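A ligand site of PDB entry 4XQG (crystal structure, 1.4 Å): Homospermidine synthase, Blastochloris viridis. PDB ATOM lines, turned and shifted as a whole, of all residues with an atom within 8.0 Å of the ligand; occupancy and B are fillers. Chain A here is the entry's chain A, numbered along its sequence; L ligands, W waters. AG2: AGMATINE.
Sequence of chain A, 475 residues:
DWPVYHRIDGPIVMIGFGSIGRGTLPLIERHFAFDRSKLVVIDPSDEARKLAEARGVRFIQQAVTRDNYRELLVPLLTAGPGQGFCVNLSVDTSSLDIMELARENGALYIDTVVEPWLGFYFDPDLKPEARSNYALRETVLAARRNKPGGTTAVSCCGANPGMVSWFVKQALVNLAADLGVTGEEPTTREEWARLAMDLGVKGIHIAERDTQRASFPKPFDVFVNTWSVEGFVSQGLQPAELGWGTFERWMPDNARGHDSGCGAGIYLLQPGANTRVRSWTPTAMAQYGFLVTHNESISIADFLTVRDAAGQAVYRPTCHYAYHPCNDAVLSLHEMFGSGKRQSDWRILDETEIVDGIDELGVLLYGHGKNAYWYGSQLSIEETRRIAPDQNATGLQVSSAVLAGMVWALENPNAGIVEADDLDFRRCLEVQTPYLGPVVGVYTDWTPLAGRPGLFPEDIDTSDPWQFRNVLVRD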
ATOM      1  N   ARG A 137      14.361  22.380  28.028  1.00  0.00           N
ATOM      2  CA  ARG A 137      12.897  22.462  27.986  1.00  0.00           C
ATOM      3  C   ARG A 137      12.336  21.568  26.851  1.00  0.00           C
ATOM      4  O   ARG A 137      11.277  20.951  27.006  1.00  0.00           O
ATOM      5  CB  ARG A 137      12.455  23.912  27.826  1.00  0.00           C
ATOM      6  CG  ARG A 137      10.964  24.066  27.630  1.00  0.00           C
ATOM      7  CD  ARG A 137      10.580  25.521  27.644  1.00  0.00           C
ATOM      8  NE  ARG A 137       9.134  25.682  27.494  1.00  0.00           N
ATOM      9  CZ  ARG A 137       8.512  25.864  26.322  1.00  0.00           C
ATOM     10  NH1 ARG A 137       9.199  25.951  25.188  1.00  0.00           N
ATOM     11  NH2 ARG A 137       7.203  25.997  26.292  1.00  0.00           N
ATOM     12  N   LEU A 141       9.071  18.959  26.574  1.00  0.00           N
ATOM     13  CA  LEU A 141       8.042  19.010  25.538  1.00  0.00           C
ATOM     14  C   LEU A 141       7.937  17.709  24.758  1.00  0.00           C
ATOM     15  O   LEU A 141       6.839  17.278  24.430  1.00  0.00           O
ATOM     16  CB  LEU A 141       8.277  20.184  24.567  1.00  0.00           C
ATOM     17  CG  LEU A 141       8.334  21.586  25.172  1.00  0.00           C
ATOM     18  CD1 LEU A 141       8.284  22.661  24.107  1.00  0.00           C
ATOM     19  CD2 LEU A 141       7.270  21.847  26.216  1.00  0.00           C
ATOM     20  N   ARG A 144       6.162  15.121  26.872  1.00  0.00           N
ATOM     21  CA  ARG A 144       4.726  15.361  26.799  1.00  0.00           C
ATOM     22  C   ARG A 144       4.096  14.854  25.507  1.00  0.00           C
ATOM     23  O   ARG A 144       3.000  14.300  25.532  1.00  0.00           O
ATOM     24  CB  ARG A 144       4.419  16.836  27.010  1.00  0.00           C
ATOM     25  CG  ARG A 144       2.949  17.168  26.821  1.00  0.00           C
ATOM     26  CD  ARG A 144       2.619  18.495  27.462  1.00  0.00           C
ATOM     27  NE  ARG A 144       3.212  19.619  26.761  1.00  0.00           N
ATOM     28  CZ  ARG A 144       3.320  20.846  27.283  1.00  0.00           C
ATOM     29  NH1 ARG A 144       2.919  21.103  28.523  1.00  0.00           N
ATOM     30  NH2 ARG A 144       3.844  21.832  26.545  1.00  0.00           N
ATOM     31  N   PRO A 148       0.985  11.908  26.272  1.00  0.00           N
ATOM     32  CA  PRO A 148       0.004  12.959  26.558  1.00  0.00           C
ATOM     33  C   PRO A 148      -0.887  12.582  27.726  1.00  0.00           C
ATOM     34  O   PRO A 148      -1.175  11.406  27.953  1.00  0.00           O
ATOM     35  CB  PRO A 148      -0.803  13.075  25.266  1.00  0.00           C
ATOM     36  CG  PRO A 148      -0.110  12.256  24.264  1.00  0.00           C
ATOM     37  CD  PRO A 148       0.795  11.323  24.928  1.00  0.00           C
ATOM     38  N   GLY A 149      -1.345  13.588  28.469  1.00  0.00           N
ATOM     39  CA  GLY A 149      -2.209  13.334  29.616  1.00  0.00           C
ATOM     40  C   GLY A 149      -1.511  12.525  30.695  1.00  0.00           C
ATOM     41  O   GLY A 149      -0.286  12.536  30.806  1.00  0.00           O
ATOM     42  N   LYS A 169      -0.224  36.934  32.730  1.00  0.00           N
ATOM     43  CA  LYS A 169      -1.651  36.899  32.475  1.00  0.00           C
ATOM     44  C   LYS A 169      -2.380  38.047  33.170  1.00  0.00           C
ATOM     45  O   LYS A 169      -3.197  38.742  32.552  1.00  0.00           O
ATOM     46  CB  LYS A 169      -2.244  35.549  32.855  1.00  0.00           C
ATOM     47  CG  LYS A 169      -1.878  34.423  31.893  1.00  0.00           C
ATOM     48  CD  LYS A 169      -2.702  33.166  32.155  1.00  0.00           C
ATOM     49  CE  LYS A 169      -2.471  32.085  31.106  1.00  0.00           C
ATOM     50  NZ  LYS A 169      -1.167  31.403  31.295  1.00  0.00           N
ATOM     51  N   ARG A 189      -5.011  29.046  25.286  1.00  0.00           N
ATOM     52  CA  ARG A 189      -3.682  29.537  24.956  1.00  0.00           C
ATOM     53  C   ARG A 189      -3.733  30.467  23.756  1.00  0.00           C
ATOM     54  O   ARG A 189      -3.114  31.542  23.759  1.00  0.00           O
ATOM     55  CB  ARG A 189      -2.712  28.381  24.671  1.00  0.00           C
ATOM     56  CG  ARG A 189      -1.356  28.820  24.126  1.00  0.00           C
ATOM     57  CD  ARG A 189      -0.420  27.632  23.839  1.00  0.00           C
ATOM     58  NE  ARG A 189      -1.086  26.565  23.114  1.00  0.00           N
ATOM     59  CZ  ARG A 189      -1.247  26.545  21.783  1.00  0.00           C
ATOM     60  NH1 ARG A 189      -0.788  27.540  21.039  1.00  0.00           N
ATOM     61  NH2 ARG A 189      -1.881  25.528  21.215  1.00  0.00           N
ATOM     62  N   CYS A 262      10.269  24.375  19.633  1.00  0.00           N
ATOM     63  CA  CYS A 262       9.096  25.258  19.549  1.00  0.00           C
ATOM     64  C   CYS A 262       9.319  26.515  18.713  1.00  0.00           C
ATOM     65  O   CYS A 262       8.347  27.141  18.288  1.00  0.00           O
ATOM     66  CB  CYS A 262       8.613  25.627  20.955  1.00  0.00           C
ATOM     67  SG  CYS A 262       9.696  26.752  21.838  1.00  0.00           S
ATOM     68  N   ILE A 298      11.798  31.328  27.512  1.00  0.00           N
ATOM     69  CA  ILE A 298      11.286  30.544  26.394  1.00  0.00           C
ATOM     70  C   ILE A 298       9.797  30.207  26.547  1.00  0.00           C
ATOM     71  O   ILE A 298       9.028  30.323  25.598  1.00  0.00           O
ATOM     72  CB  ILE A 298      12.083  29.238  26.213  1.00  0.00           C
ATOM     73  CG1 ILE A 298      13.590  29.522  26.176  1.00  0.00           C
ATOM     74  CG2 ILE A 298      11.632  28.513  24.948  1.00  0.00           C
ATOM     75  CD1 ILE A 298      14.034  30.502  25.108  1.00  0.00           C
ATOM     76  N   SER A 299       9.370  29.756  27.733  1.00  0.00           N
ATOM     77  CA  SER A 299       7.998  29.257  27.877  1.00  0.00           C
ATOM     78  C   SER A 299       6.930  30.342  27.682  1.00  0.00           C
ATOM     79  O   SER A 299       5.886  30.075  27.108  1.00  0.00           O
ATOM     80  CB  SER A 299       7.787  28.504  29.211  1.00  0.00           C
ATOM     81  OG  SER A 299       7.471  29.377  30.278  1.00  0.00           O
ATOM     82  N   ILE A 300       7.208  31.558  28.148  1.00  0.00           N
ATOM     83  CA  ILE A 300       6.231  32.651  28.011  1.00  0.00           C
ATOM     84  C   ILE A 300       6.146  33.080  26.551  1.00  0.00           C
ATOM     85  O   ILE A 300       5.056  33.300  26.018  1.00  0.00           O
ATOM     86  CB  ILE A 300       6.576  33.840  28.928  1.00  0.00           C
ATOM     87  CG1 ILE A 300       6.398  33.420  30.379  1.00  0.00           C
ATOM     88  CG2 ILE A 300       5.757  35.108  28.585  1.00  0.00           C
ATOM     89  CD1 ILE A 300       7.027  34.397  31.388  1.00  0.00           C
ATOM     90  N   ALA A 301       7.299  33.211  25.886  1.00  0.00           N
ATOM     91  CA  ALA A 301       7.306  33.568  24.476  1.00  0.00           C
ATOM     92  C   ALA A 301       6.599  32.512  23.616  1.00  0.00           C
ATOM     93  O   ALA A 301       5.818  32.840  22.740  1.00  0.00           O
ATOM     94  CB  ALA A 301       8.746  33.799  23.981  1.00  0.00           C
ATOM     95  N   ASP A 302       6.824  31.241  23.921  1.00  0.00           N
ATOM     96  CA  ASP A 302       6.147  30.131  23.248  1.00  0.00           C
ATOM     97  C   ASP A 302       4.643  30.189  23.499  1.00  0.00           C
ATOM     98  O   ASP A 302       3.844  30.129  22.548  1.00  0.00           O
ATOM     99  CB  ASP A 302       6.748  28.814  23.759  1.00  0.00           C
ATOM    100  CG  ASP A 302       6.247  27.577  23.026  1.00  0.00           C
ATOM    101  OD1 ASP A 302       5.768  27.668  21.861  1.00  0.00           O
ATOM    102  OD2 ASP A 302       6.369  26.461  23.597  1.00  0.00           O
ATOM    103  N   PHE A 303       4.254  30.304  24.768  1.00  0.00           N
ATOM    104  CA  PHE A 303       2.852  30.368  25.129  1.00  0.00           C
ATOM    105  C   PHE A 303       2.089  31.472  24.381  1.00  0.00           C
ATOM    106  O   PHE A 303       0.961  31.276  23.933  1.00  0.00           O
ATOM    107  CB  PHE A 303       2.709  30.542  26.649  1.00  0.00           C
ATOM    108  CG  PHE A 303       1.282  30.486  27.123  1.00  0.00           C
ATOM    109  CD1 PHE A 303       0.639  29.261  27.278  1.00  0.00           C
ATOM    110  CD2 PHE A 303       0.570  31.643  27.370  1.00  0.00           C
ATOM    111  CE1 PHE A 303      -0.670  29.210  27.706  1.00  0.00           C
ATOM    112  CE2 PHE A 303      -0.731  31.593  27.809  1.00  0.00           C
ATOM    113  CZ  PHE A 303      -1.363  30.394  27.955  1.00  0.00           C
ATOM    114  N   LEU A 304       2.725  32.622  24.259  1.00  0.00           N
ATOM    115  CA  LEU A 304       2.123  33.796  23.631  1.00  0.00           C
ATOM    116  C   LEU A 304       2.387  33.894  22.127  1.00  0.00           C
ATOM    117  O   LEU A 304       2.271  34.957  21.545  1.00  0.00           O
ATOM    118  CB  LEU A 304       2.568  35.074  24.341  1.00  0.00           C
ATOM    119  CG  LEU A 304       2.094  35.174  25.797  1.00  0.00           C
ATOM    120  CD1 LEU A 304       2.628  36.452  26.438  1.00  0.00           C
ATOM    121  CD2 LEU A 304       0.572  35.113  25.935  1.00  0.00           C
ATOM    122  N   THR A 305       2.718  32.775  21.490  1.00  0.00           N
ATOM    123  CA  THR A 305       2.916  32.760  20.033  1.00  0.00           C
ATOM    124  C   THR A 305       1.595  32.579  19.297  1.00  0.00           C
ATOM    125  O   THR A 305       0.797  31.683  19.603  1.00  0.00           O
ATOM    126  CB  THR A 305       3.887  31.625  19.635  1.00  0.00           C
ATOM    127  OG1 THR A 305       5.190  31.906  20.168  1.00  0.00           O
ATOM    128  CG2 THR A 305       4.026  31.484  18.135  1.00  0.00           C
ATOM    129  N   TRP A 408      -2.734  23.415  42.876  1.00  0.00           N
ATOM    130  CA  TRP A 408      -3.296  23.253  41.548  1.00  0.00           C
ATOM    131  C   TRP A 408      -3.209  21.789  41.085  1.00  0.00           C
ATOM    132  O   TRP A 408      -4.195  21.226  40.571  1.00  0.00           O
ATOM    133  CB  TRP A 408      -2.653  24.218  40.541  1.00  0.00           C
ATOM    134  CG  TRP A 408      -3.398  24.216  39.234  1.00  0.00           C
ATOM    135  CD1 TRP A 408      -4.422  25.036  38.867  1.00  0.00           C
ATOM    136  CD2 TRP A 408      -3.212  23.302  38.135  1.00  0.00           C
ATOM    137  NE1 TRP A 408      -4.872  24.716  37.612  1.00  0.00           N
ATOM    138  CE2 TRP A 408      -4.147  23.659  37.133  1.00  0.00           C
ATOM    139  CE3 TRP A 408      -2.356  22.224  37.892  1.00  0.00           C
ATOM    140  CZ2 TRP A 408      -4.250  22.981  35.911  1.00  0.00           C
ATOM    141  CZ3 TRP A 408      -2.458  21.547  36.670  1.00  0.00           C
ATOM    142  CH2 TRP A 408      -3.390  21.936  35.699  1.00  0.00           C
ATOM    143  N   ALA A 415      -3.858  16.132  34.492  1.00  0.00           N
ATOM    144  CA  ALA A 415      -3.597  17.138  33.471  1.00  0.00           C
ATOM    145  C   ALA A 415      -2.322  16.888  32.660  1.00  0.00           C
ATOM    146  O   ALA A 415      -2.015  17.631  31.724  1.00  0.00           O
ATOM    147  CB  ALA A 415      -3.545  18.539  34.123  1.00  0.00           C
ATOM    148  N   GLY A 416      -1.573  15.856  33.021  1.00  0.00           N
ATOM    149  CA  GLY A 416      -0.316  15.569  32.360  1.00  0.00           C
ATOM    150  C   GLY A 416       0.796  16.565  32.678  1.00  0.00           C
ATOM    151  O   GLY A 416       0.766  17.267  33.698  1.00  0.00           O
ATOM    152  N   ILE A 417       1.802  16.566  31.823  1.00  0.00           N
ATOM    153  CA  ILE A 417       2.950  17.453  31.997  1.00  0.00           C
ATOM    154  C   ILE A 417       2.518  18.879  31.643  1.00  0.00           C
ATOM    155  O   ILE A 417       2.036  19.155  30.519  1.00  0.00           O
ATOM    156  CB  ILE A 417       4.124  17.010  31.121  1.00  0.00           C
ATOM    157  CG1 ILE A 417       4.665  15.670  31.606  1.00  0.00           C
ATOM    158  CG2 ILE A 417       5.231  18.038  31.098  1.00  0.00           C
ATOM    159  CD1 ILE A 417       5.504  14.977  30.578  1.00  0.00           C
ATOM    160  N   VAL A 418       2.685  19.788  32.593  1.00  0.00           N
ATOM    161  CA  VAL A 418       2.276  21.171  32.395  1.00  0.00           C
ATOM    162  C   VAL A 418       3.348  22.129  32.886  1.00  0.00           C
ATOM    163  O   VAL A 418       4.160  21.779  33.741  1.00  0.00           O
ATOM    164  CB  VAL A 418       0.956  21.491  33.134  1.00  0.00           C
ATOM    165  CG1 VAL A 418      -0.256  20.825  32.450  1.00  0.00           C
ATOM    166  CG2 VAL A 418       1.034  21.082  34.631  1.00  0.00           C
ATOM    167  N   GLU A 419       3.343  23.337  32.328  1.00  0.00           N
ATOM    168  CA  GLU A 419       4.196  24.427  32.812  1.00  0.00           C
ATOM    169  C   GLU A 419       3.321  25.428  33.542  1.00  0.00           C
ATOM    170  O   GLU A 419       2.087  25.332  33.499  1.00  0.00           O
ATOM    171  CB  GLU A 419       4.926  25.118  31.664  1.00  0.00           C
ATOM    172  CG  GLU A 419       6.119  24.296  31.142  1.00  0.00           C
ATOM    173  CD  GLU A 419       6.805  24.937  29.947  1.00  0.00           C
ATOM    174  OE1 GLU A 419       6.113  25.298  28.975  1.00  0.00           O
ATOM    175  OE2 GLU A 419       8.043  25.083  29.995  1.00  0.00           O
ATOM    176  N   ALA A 420       3.946  26.399  34.185  1.00  0.00           N
ATOM    177  CA  ALA A 420       3.182  27.391  34.916  1.00  0.00           C
ATOM    178  C   ALA A 420       2.227  28.171  33.996  1.00  0.00           C
ATOM    179  O   ALA A 420       1.197  28.652  34.455  1.00  0.00           O
ATOM    180  CB  ALA A 420       4.112  28.346  35.632  1.00  0.00           C
ATOM    181  N   ASP A 421       2.574  28.277  32.718  1.00  0.00           N
ATOM    182  CA  ASP A 421       1.727  28.932  31.727  1.00  0.00           C
ATOM    183  C   ASP A 421       0.407  28.185  31.488  1.00  0.00           C
ATOM    184  O   ASP A 421      -0.544  28.769  30.982  1.00  0.00           O
ATOM    185  CB  ASP A 421       2.473  29.102  30.397  1.00  0.00           C
ATOM    186  CG  ASP A 421       3.828  29.715  30.587  1.00  0.00           C
ATOM    187  OD1 ASP A 421       3.896  30.949  30.759  1.00  0.00           O
ATOM    188  OD2 ASP A 421       4.814  28.972  30.584  1.00  0.00           O
ATOM    189  N   ASP A 422       0.365  26.903  31.857  1.00  0.00           N
ATOM    190  CA  ASP A 422      -0.810  26.076  31.606  1.00  0.00           C
ATOM    191  C   ASP A 422      -1.796  26.037  32.774  1.00  0.00           C
ATOM    192  O   ASP A 422      -2.917  25.546  32.634  1.00  0.00           O
ATOM    193  CB  ASP A 422      -0.343  24.663  31.267  1.00  0.00           C
ATOM    194  CG  ASP A 422       0.517  24.612  30.034  1.00  0.00           C
ATOM    195  OD1 ASP A 422       0.118  25.189  29.003  1.00  0.00           O
ATOM    196  OD2 ASP A 422       1.625  24.008  30.090  1.00  0.00           O
ATOM    197  N   LEU A 423      -1.373  26.551  33.924  1.00  0.00           N
ATOM    198  CA  LEU A 423      -2.208  26.457  35.116  1.00  0.00           C
ATOM    199  C   LEU A 423      -3.252  27.567  35.163  1.00  0.00           C
ATOM    200  O   LEU A 423      -3.118  28.579  34.460  1.00  0.00           O
ATOM    201  CB  LEU A 423      -1.356  26.531  36.375  1.00  0.00           C
ATOM    202  CG  LEU A 423      -0.069  25.736  36.379  1.00  0.00           C
ATOM    203  CD1 LEU A 423       0.554  25.789  37.778  1.00  0.00           C
ATOM    204  CD2 LEU A 423      -0.239  24.286  35.895  1.00  0.00           C
HETATM  205  N   AG2 L   1      -1.598  20.597  28.143  1.00  0.00           N
HETATM  206  CA  AG2 L   1      -0.364  21.257  27.850  1.00  0.00           C
HETATM  207  CB  AG2 L   1      -0.643  22.428  26.940  1.00  0.00           C
HETATM  208  CG  AG2 L   1       0.651  23.050  26.460  1.00  0.00           C
HETATM  209  CD  AG2 L   1       0.331  24.372  25.799  1.00  0.00           C
HETATM  210  NE  AG2 L   1       1.491  24.933  25.181  1.00  0.00           N
HETATM  211  CZ  AG2 L   1       2.321  25.817  25.900  1.00  0.00           C
HETATM  212  NH1 AG2 L   1       3.466  26.377  25.258  1.00  0.00           N
HETATM  213  NH2 AG2 L   1       2.024  26.083  27.163  1.00  0.00           N
HETATM  214  O   HOH W   1      -0.395  18.247  29.665  1.00  0.00           O
HETATM  215  O   HOH W   2       2.650  25.409  22.404  1.00  0.00           O
HETATM  216  O   HOH W   3      -3.244  19.998  26.024  1.00  0.00           O
HETATM  217  O   HOH W   4      -3.689  19.570  30.695  1.00  0.00           O
HETATM  218  O   HOH W   5      -3.168  22.543  29.719  1.00  0.00           O
HETATM  219  O   HOH W   6       3.848  23.859  28.523  1.00  0.00           O
HETATM  220  O   HOH W   7       4.589  27.544  27.503  1.00  0.00           O
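OD1 of Asp 422 lies within salt-bridge range of NH2 of the ligand (2.8 Å).
The side-chain carboxylate (OD2) of Asp 302 lies within salt-bridge range of a nitrogen (NH1) of the ligand, at 3.3 Å.
The side-chain carboxylate (OD2) of Asp 422 is in salt-bridge range of the guanidinium group (NH1) of Arg 144 (3.5 Å).
The side-chain carboxylate (OD2) of Asp 422 sits at hydrogen-bond distance from the backbone NH (N) of Glu 419 (2.9 Å).
OD2 of Asp 302 lies within salt-bridge range of NH2 of Arg 137, at 2.9 Å.
OD2 of Asp 302 lies close to SG of Cys 262 (3.8 Å).
O of Asp 302 lies within hydrogen-bond range of OG1 of Thr 305 (3.3 Å).
The backbone carbonyl oxygen (O) of Ile 417 is in hydrogen-bond range of the guanidinium group (NH1) of Arg 144, at 2.9 Å.
NE of Arg 137 lies within salt-bridge range of OE2 of Glu 419 (2.8 Å).
The side-chain sulfur (SG) of Cys 262 sits at hydrogen-bond distance from the guanidinium group (NH1) of Arg 137, at 3.5 Å.
NH2 of Arg 137 touches NH1 of the ligand, 3.9 Å away.
NH1 of Arg 144 touches CA of the ligand, 3.4 Å away.
CD of Arg 189 touches NE of the ligand (3.6 Å).
Phe 303 touches the ligand.
Hydrophobic or aromatic side chains that line the ligand: Phe 303.
Six residues have an atom within 4 Å of the ligand: Arg 137, Arg 144, Arg 189, Asp 302, Phe 303 and Asp 422.
The nearest printed residue that does not touch the ligand is Ile 417 (4.2 Å).
Water W1 lies within hydrogen-bond range of O of Ala 415, O of Ile 417 and N of the ligand.
Water W6 lies within hydrogen-bond range of OE1 of Glu 419 (2.7 Å), OD2 of Asp 422 (2.7 Å), NH2 of Arg 144 (2.8 Å) and NH2 of the ligand (3.2 Å).
Water W4 lies within hydrogen-bond range of O of Ala 415 and N of the ligand.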
